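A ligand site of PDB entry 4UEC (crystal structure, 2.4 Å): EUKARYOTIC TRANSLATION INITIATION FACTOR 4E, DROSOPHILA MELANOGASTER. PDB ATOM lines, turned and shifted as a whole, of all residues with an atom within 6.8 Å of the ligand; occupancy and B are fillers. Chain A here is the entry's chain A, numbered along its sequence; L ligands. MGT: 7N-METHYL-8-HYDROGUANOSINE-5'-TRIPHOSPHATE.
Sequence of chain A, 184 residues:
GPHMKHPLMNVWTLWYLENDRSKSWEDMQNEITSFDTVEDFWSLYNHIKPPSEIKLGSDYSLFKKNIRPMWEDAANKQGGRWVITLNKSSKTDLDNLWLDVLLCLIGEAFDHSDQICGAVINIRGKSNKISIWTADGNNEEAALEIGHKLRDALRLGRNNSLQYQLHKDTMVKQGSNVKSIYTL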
ATOM      1  N   LEU A  17     -23.462  22.891  11.786  1.00  0.00           N
ATOM      2  CA  LEU A  17     -22.497  22.693  10.715  1.00  0.00           C
ATOM      3  C   LEU A  17     -22.849  23.543   9.504  1.00  0.00           C
ATOM      4  O   LEU A  17     -24.004  23.626   9.108  1.00  0.00           O
ATOM      5  CB  LEU A  17     -22.439  21.218  10.320  1.00  0.00           C
ATOM      6  CG  LEU A  17     -21.587  20.868   9.095  1.00  0.00           C
ATOM      7  CD1 LEU A  17     -20.841  19.563   9.308  1.00  0.00           C
ATOM      8  CD2 LEU A  17     -22.442  20.786   7.836  1.00  0.00           C
ATOM      9  N   TRP A  25     -14.872  18.227   6.727  1.00  0.00           N
ATOM     10  CA  TRP A  25     -16.156  18.034   7.395  1.00  0.00           C
ATOM     11  C   TRP A  25     -16.083  18.248   8.904  1.00  0.00           C
ATOM     12  O   TRP A  25     -17.028  18.744   9.518  1.00  0.00           O
ATOM     13  CB  TRP A  25     -16.699  16.631   7.108  1.00  0.00           C
ATOM     14  CG  TRP A  25     -18.053  16.391   7.687  1.00  0.00           C
ATOM     15  CD1 TRP A  25     -19.257  16.594   7.078  1.00  0.00           C
ATOM     16  CD2 TRP A  25     -18.352  15.902   9.003  1.00  0.00           C
ATOM     17  NE1 TRP A  25     -20.281  16.261   7.932  1.00  0.00           N
ATOM     18  CE2 TRP A  25     -19.752  15.834   9.116  1.00  0.00           C
ATOM     19  CE3 TRP A  25     -17.560  15.512  10.083  1.00  0.00           C
ATOM     20  CZ2 TRP A  25     -20.379  15.398  10.287  1.00  0.00           C
ATOM     21  CZ3 TRP A  25     -18.188  15.076  11.236  1.00  0.00           C
ATOM     22  CH2 TRP A  25     -19.588  15.020  11.331  1.00  0.00           C
ATOM     23  N   GLU A  26     -14.948  17.882   9.501  1.00  0.00           N
ATOM     24  CA  GLU A  26     -14.768  18.053  10.937  1.00  0.00           C
ATOM     25  C   GLU A  26     -14.678  19.533  11.317  1.00  0.00           C
ATOM     26  O   GLU A  26     -15.081  19.939  12.401  1.00  0.00           O
ATOM     27  CB  GLU A  26     -13.519  17.308  11.407  1.00  0.00           C
ATOM     28  CG  GLU A  26     -13.256  17.421  12.908  1.00  0.00           C
ATOM     29  CD  GLU A  26     -12.078  16.578  13.363  1.00  0.00           C
ATOM     30  OE1 GLU A  26     -11.578  15.770  12.557  1.00  0.00           O
ATOM     31  OE2 GLU A  26     -11.652  16.719  14.533  1.00  0.00           O
ATOM     32  N   GLN A  29     -18.099  21.727  11.568  1.00  0.00           N
ATOM     33  CA  GLN A  29     -18.873  21.678  12.805  1.00  0.00           C
ATOM     34  C   GLN A  29     -18.561  22.850  13.723  1.00  0.00           C
ATOM     35  O   GLN A  29     -17.413  23.269  13.827  1.00  0.00           O
ATOM     36  CB  GLN A  29     -18.622  20.362  13.543  1.00  0.00           C
ATOM     37  CG  GLN A  29     -19.243  19.144  12.885  1.00  0.00           C
ATOM     38  CD  GLN A  29     -20.759  19.136  12.989  1.00  0.00           C
ATOM     39  OE1 GLN A  29     -21.359  20.010  13.621  1.00  0.00           O
ATOM     40  NE2 GLN A  29     -21.382  18.136  12.375  1.00  0.00           N
ATOM     41  N   ASP A  59     -26.168  21.454   8.982  1.00  0.00           N
ATOM     42  CA  ASP A  59     -26.745  20.489   9.908  1.00  0.00           C
ATOM     43  C   ASP A  59     -26.995  21.123  11.270  1.00  0.00           C
ATOM     44  O   ASP A  59     -26.253  22.010  11.699  1.00  0.00           O
ATOM     45  CB  ASP A  59     -25.837  19.273  10.098  1.00  0.00           C
ATOM     46  CG  ASP A  59     -25.443  18.600   8.800  1.00  0.00           C
ATOM     47  OD1 ASP A  59     -26.164  18.747   7.792  1.00  0.00           O
ATOM     48  OD2 ASP A  59     -24.414  17.902   8.800  1.00  0.00           O
ATOM     49  N   PRO A  69     -20.839  14.787  17.410  1.00  0.00           N
ATOM     50  CA  PRO A  69     -21.704  14.140  16.421  1.00  0.00           C
ATOM     51  C   PRO A  69     -20.893  13.510  15.293  1.00  0.00           C
ATOM     52  O   PRO A  69     -21.030  13.891  14.126  1.00  0.00           O
ATOM     53  CB  PRO A  69     -22.570  15.291  15.928  1.00  0.00           C
ATOM     54  CG  PRO A  69     -21.694  16.485  16.045  1.00  0.00           C
ATOM     55  CD  PRO A  69     -20.847  16.255  17.260  1.00  0.00           C
ATOM     56  N   MET A  70     -20.044  12.537  15.649  1.00  0.00           N
ATOM     57  CA  MET A  70     -19.154  11.893  14.683  1.00  0.00           C
ATOM     58  C   MET A  70     -19.123  10.383  14.886  1.00  0.00           C
ATOM     59  O   MET A  70     -19.279   9.891  15.996  1.00  0.00           O
ATOM     60  CB  MET A  70     -17.734  12.443  14.805  1.00  0.00           C
ATOM     61  CG  MET A  70     -17.633  13.951  14.734  1.00  0.00           C
ATOM     62  SD  MET A  70     -15.944  14.543  15.001  1.00  0.00           S
ATOM     63  CE  MET A  70     -15.064  13.707  13.676  1.00  0.00           C
ATOM     64  N   TRP A  71     -18.902   9.653  13.794  1.00  0.00           N
ATOM     65  CA  TRP A  71     -18.683   8.212  13.887  1.00  0.00           C
ATOM     66  C   TRP A  71     -17.455   7.945  14.742  1.00  0.00           C
ATOM     67  O   TRP A  71     -17.403   6.978  15.507  1.00  0.00           O
ATOM     68  CB  TRP A  71     -18.485   7.571  12.513  1.00  0.00           C
ATOM     69  CG  TRP A  71     -19.488   7.947  11.472  1.00  0.00           C
ATOM     70  CD1 TRP A  71     -20.842   7.900  11.591  1.00  0.00           C
ATOM     71  CD2 TRP A  71     -19.214   8.373  10.127  1.00  0.00           C
ATOM     72  NE1 TRP A  71     -21.435   8.294  10.410  1.00  0.00           N
ATOM     73  CE2 TRP A  71     -20.455   8.588   9.504  1.00  0.00           C
ATOM     74  CE3 TRP A  71     -18.040   8.601   9.416  1.00  0.00           C
ATOM     75  CZ2 TRP A  71     -20.555   9.024   8.184  1.00  0.00           C
ATOM     76  CZ3 TRP A  71     -18.140   9.037   8.096  1.00  0.00           C
ATOM     77  CH2 TRP A  71     -19.389   9.242   7.503  1.00  0.00           C
ATOM     78  N   GLU A  72     -16.468   8.830  14.611  1.00  0.00           N
ATOM     79  CA  GLU A  72     -15.172   8.659  15.267  1.00  0.00           C
ATOM     80  C   GLU A  72     -15.282   8.738  16.785  1.00  0.00           C
ATOM     81  O   GLU A  72     -14.407   8.235  17.503  1.00  0.00           O
ATOM     82  CB  GLU A  72     -14.186   9.731  14.777  1.00  0.00           C
ATOM     83  CG  GLU A  72     -13.744   9.563  13.331  1.00  0.00           C
ATOM     84  CD  GLU A  72     -14.781  10.040  12.328  1.00  0.00           C
ATOM     85  OE1 GLU A  72     -15.928  10.299  12.727  1.00  0.00           O
ATOM     86  OE2 GLU A  72     -14.440  10.159  11.130  1.00  0.00           O
ATOM     87  N   ASP A  73     -16.337   9.363  17.274  1.00  0.00           N
ATOM     88  CA  ASP A  73     -16.537   9.493  18.715  1.00  0.00           C
ATOM     89  C   ASP A  73     -16.741   8.108  19.323  1.00  0.00           C
ATOM     90  O   ASP A  73     -17.423   7.258  18.758  1.00  0.00           O
ATOM     91  CB  ASP A  73     -17.735  10.392  19.021  1.00  0.00           C
ATOM     92  CG  ASP A  73     -17.664  10.992  20.406  1.00  0.00           C
ATOM     93  OD1 ASP A  73     -18.053  10.311  21.383  1.00  0.00           O
ATOM     94  OD2 ASP A  73     -17.233  12.154  20.522  1.00  0.00           O
ATOM     95  N   ARG A  81     -27.783   4.654  13.406  1.00  0.00           N
ATOM     96  CA  ARG A  81     -28.712   5.779  13.374  1.00  0.00           C
ATOM     97  C   ARG A  81     -30.026   5.427  12.689  1.00  0.00           C
ATOM     98  O   ARG A  81     -30.046   4.836  11.618  1.00  0.00           O
ATOM     99  CB  ARG A  81     -28.071   6.980  12.659  1.00  0.00           C
ATOM    100  CG  ARG A  81     -27.569   6.691  11.250  1.00  0.00           C
ATOM    101  CD  ARG A  81     -27.220   7.972  10.513  1.00  0.00           C
ATOM    102  NE  ARG A  81     -26.816   7.708   9.135  1.00  0.00           N
ATOM    103  CZ  ARG A  81     -26.740   8.640   8.185  1.00  0.00           C
ATOM    104  NH1 ARG A  81     -27.052   9.901   8.456  1.00  0.00           N
ATOM    105  NH2 ARG A  81     -26.373   8.300   6.956  1.00  0.00           N
ATOM    106  N   VAL A 120     -29.507  14.192  14.473  1.00  0.00           N
ATOM    107  CA  VAL A 120     -28.950  15.082  13.467  1.00  0.00           C
ATOM    108  C   VAL A 120     -29.979  15.349  12.371  1.00  0.00           C
ATOM    109  O   VAL A 120     -30.583  14.412  11.857  1.00  0.00           O
ATOM    110  CB  VAL A 120     -27.670  14.495  12.819  1.00  0.00           C
ATOM    111  CG1 VAL A 120     -27.090  15.458  11.789  1.00  0.00           C
ATOM    112  CG2 VAL A 120     -26.641  14.161  13.884  1.00  0.00           C
ATOM    113  N   ASN A 122     -30.205  17.053   8.577  1.00  0.00           N
ATOM    114  CA  ASN A 122     -29.445  17.526   7.426  1.00  0.00           C
ATOM    115  C   ASN A 122     -30.360  18.274   6.463  1.00  0.00           C
ATOM    116  O   ASN A 122     -31.396  17.742   6.047  1.00  0.00           O
ATOM    117  CB  ASN A 122     -28.772  16.367   6.695  1.00  0.00           C
ATOM    118  CG  ASN A 122     -27.908  15.515   7.605  1.00  0.00           C
ATOM    119  OD1 ASN A 122     -26.783  15.869   7.936  1.00  0.00           O
ATOM    120  ND2 ASN A 122     -28.438  14.358   7.998  1.00  0.00           N
ATOM    121  N   ARG A 124     -30.568  19.581   2.762  1.00  0.00           N
ATOM    122  CA  ARG A 124     -29.907  19.335   1.486  1.00  0.00           C
ATOM    123  C   ARG A 124     -30.754  19.731   0.283  1.00  0.00           C
ATOM    124  O   ARG A 124     -30.394  19.456  -0.863  1.00  0.00           O
ATOM    125  CB  ARG A 124     -29.527  17.846   1.374  1.00  0.00           C
ATOM    126  CG  ARG A 124     -28.575  17.361   2.462  1.00  0.00           C
ATOM    127  CD  ARG A 124     -27.205  17.999   2.327  1.00  0.00           C
ATOM    128  NE  ARG A 124     -26.287  17.543   3.358  1.00  0.00           N
ATOM    129  CZ  ARG A 124     -26.251  18.008   4.598  1.00  0.00           C
ATOM    130  NH1 ARG A 124     -27.082  18.971   4.985  1.00  0.00           N
ATOM    131  NH2 ARG A 124     -25.372  17.524   5.472  1.00  0.00           N
ATOM    132  N   SER A 127     -33.507  16.505  -0.526  1.00  0.00           N
ATOM    133  CA  SER A 127     -34.134  15.730   0.521  1.00  0.00           C
ATOM    134  C   SER A 127     -33.496  16.032   1.875  1.00  0.00           C
ATOM    135  O   SER A 127     -32.288  15.915   2.036  1.00  0.00           O
ATOM    136  CB  SER A 127     -34.025  14.232   0.216  1.00  0.00           C
ATOM    137  OG  SER A 127     -34.726  13.470   1.193  1.00  0.00           O
ATOM    138  N   LYS A 129     -32.898  15.069   5.789  1.00  0.00           N
ATOM    139  CA  LYS A 129     -32.793  13.852   6.576  1.00  0.00           C
ATOM    140  C   LYS A 129     -32.699  14.162   8.064  1.00  0.00           C
ATOM    141  O   LYS A 129     -31.914  15.013   8.474  1.00  0.00           O
ATOM    142  CB  LYS A 129     -31.584  13.020   6.143  1.00  0.00           C
ATOM    143  CG  LYS A 129     -31.728  12.396   4.761  1.00  0.00           C
ATOM    144  CD  LYS A 129     -30.579  11.448   4.469  1.00  0.00           C
ATOM    145  CE  LYS A 129     -29.258  12.182   4.356  1.00  0.00           C
ATOM    146  NZ  LYS A 129     -28.152  11.268   3.944  1.00  0.00           N
ATOM    147  N   TRP A 133     -29.085   9.110  16.485  1.00  0.00           N
ATOM    148  CA  TRP A 133     -27.915   8.261  16.673  1.00  0.00           C
ATOM    149  C   TRP A 133     -28.034   7.402  17.931  1.00  0.00           C
ATOM    150  O   TRP A 133     -28.384   7.885  18.998  1.00  0.00           O
ATOM    151  CB  TRP A 133     -26.638   9.100  16.715  1.00  0.00           C
ATOM    152  CG  TRP A 133     -26.275   9.679  15.387  1.00  0.00           C
ATOM    153  CD1 TRP A 133     -27.134  10.094  14.405  1.00  0.00           C
ATOM    154  CD2 TRP A 133     -24.956   9.885  14.860  1.00  0.00           C
ATOM    155  NE1 TRP A 133     -26.437  10.554  13.319  1.00  0.00           N
ATOM    156  CE2 TRP A 133     -25.094  10.430  13.566  1.00  0.00           C
ATOM    157  CE3 TRP A 133     -23.670   9.654  15.364  1.00  0.00           C
ATOM    158  CZ2 TRP A 133     -23.998  10.758  12.786  1.00  0.00           C
ATOM    159  CZ3 TRP A 133     -22.582   9.983  14.578  1.00  0.00           C
ATOM    160  CH2 TRP A 133     -22.751  10.534  13.299  1.00  0.00           C
ATOM    161  N   THR A 170     -22.024   2.983   6.961  1.00  0.00           N
ATOM    162  CA  THR A 170     -22.242   4.307   6.387  1.00  0.00           C
ATOM    163  C   THR A 170     -20.925   4.933   5.904  1.00  0.00           C
ATOM    164  O   THR A 170     -20.918   5.758   4.991  1.00  0.00           O
ATOM    165  CB  THR A 170     -22.907   5.258   7.404  1.00  0.00           C
ATOM    166  OG1 THR A 170     -24.102   4.644   7.922  1.00  0.00           O
ATOM    167  CG2 THR A 170     -23.276   6.591   6.752  1.00  0.00           C
ATOM    168  N   MET A 171     -19.817   4.544   6.522  1.00  0.00           N
ATOM    169  CA  MET A 171     -18.503   5.050   6.140  1.00  0.00           C
ATOM    170  C   MET A 171     -18.138   4.651   4.705  1.00  0.00           C
ATOM    171  O   MET A 171     -17.319   5.314   4.065  1.00  0.00           O
ATOM    172  CB  MET A 171     -17.418   4.533   7.094  1.00  0.00           C
ATOM    173  CG  MET A 171     -17.534   5.071   8.508  1.00  0.00           C
ATOM    174  SD  MET A 171     -16.237   4.439   9.594  1.00  0.00           S
ATOM    175  CE  MET A 171     -17.091   4.408  11.168  1.00  0.00           C
HETATM  176  PG  MGT L   1     -24.693  11.087   1.516  1.00  0.00           P
HETATM  177  O1G MGT L   1     -24.665  12.286   0.577  1.00  0.00           O
HETATM  178  O2G MGT L   1     -23.525  10.142   1.571  1.00  0.00           O
HETATM  179  O3G MGT L   1     -26.093  10.515   1.615  1.00  0.00           O
HETATM  180  O3B MGT L   1     -24.711  12.044   2.980  1.00  0.00           O
HETATM  181  PB  MGT L   1     -25.447  13.406   2.781  1.00  0.00           P
HETATM  182  O1B MGT L   1     -24.769  14.569   2.117  1.00  0.00           O
HETATM  183  O2B MGT L   1     -26.944  13.380   2.791  1.00  0.00           O
HETATM  184  O3A MGT L   1     -25.406  14.224   4.416  1.00  0.00           O
HETATM  185  PA  MGT L   1     -24.194  13.638   5.200  1.00  0.00           P
HETATM  186  O1A MGT L   1     -24.145  12.143   5.354  1.00  0.00           O
HETATM  187  O2A MGT L   1     -23.558  14.552   6.213  1.00  0.00           O
HETATM  188  O5' MGT L   1     -22.742  13.697   4.059  1.00  0.00           O
HETATM  189  C5' MGT L   1     -21.998  12.596   4.392  1.00  0.00           C
HETATM  190  C4' MGT L   1     -20.552  12.998   4.143  1.00  0.00           C
HETATM  191  O4' MGT L   1     -20.136  13.838   5.240  1.00  0.00           O
HETATM  192  C3' MGT L   1     -19.718  11.700   4.165  1.00  0.00           C
HETATM  193  O3' MGT L   1     -19.359  11.434   2.845  1.00  0.00           O
HETATM  194  C2' MGT L   1     -18.499  12.073   5.015  1.00  0.00           C
HETATM  195  O2' MGT L   1     -17.426  12.506   4.237  1.00  0.00           O
HETATM  196  C1' MGT L   1     -18.985  13.299   5.858  1.00  0.00           C
HETATM  197  N9  MGT L   1     -19.340  12.850   7.218  1.00  0.00           N
HETATM  198  C8  MGT L   1     -20.733  12.724   7.706  1.00  0.00           C
HETATM  199  N7  MGT L   1     -20.610  12.281   9.065  1.00  0.00           N
HETATM  200  CM7 MGT L   1     -21.729  12.020   9.936  1.00  0.00           C
HETATM  201  C5  MGT L   1     -19.227  12.103   9.352  1.00  0.00           C
HETATM  202  C6  MGT L   1     -18.621  11.680  10.546  1.00  0.00           C
HETATM  203  O6  MGT L   1     -19.106  11.323  11.628  1.00  0.00           O
HETATM  204  N1  MGT L   1     -17.199  11.639  10.454  1.00  0.00           N
HETATM  205  C2  MGT L   1     -16.526  12.018   9.294  1.00  0.00           C
HETATM  206  N2  MGT L   1     -15.149  11.949   9.314  1.00  0.00           N
HETATM  207  N3  MGT L   1     -17.096  12.439   8.138  1.00  0.00           N
HETATM  208  C4  MGT L   1     -18.484  12.466   8.210  1.00  0.00           C
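The backbone NH of Asn 122 is in hydrogen-bond range of the backbone carbonyl oxygen of Lys 129.
The guanidinium group of Arg 124 is in hydrogen-bond range of the side-chain amide oxygen of Asn 122.
The guanidinium group (NH2) of Arg 124 is in salt-bridge range of the side-chain carboxylate (OD1) of Asp 59.
The side-chain amide oxygen (OD1) of Asn 122 sits close to the side-chain carboxylate (OD1) of Asp 59 (2.9 Å).
Residues that only touch the ligand: Met 70 (3.1 Å), Trp 25 (3.4 Å), Trp 133 (3.8 Å) and Asn 122 (3.9 Å).
The side-chain carboxylate (OE2) of Glu 72 is in hydrogen-bond range of a nitrogen (N2) of the ligand (2.6 Å).
An oxygen (O2B) of the ligand is in salt-bridge range of the side-chain amino group (NZ) of Lys 129 (2.7 Å).
The backbone NH of Trp 71 is in hydrogen-bond range of an oxygen (O6) of the ligand.
The guanidinium group (NH2) of Arg 124 is in salt-bridge range of an oxygen (O2A) of the ligand (3.6 Å).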
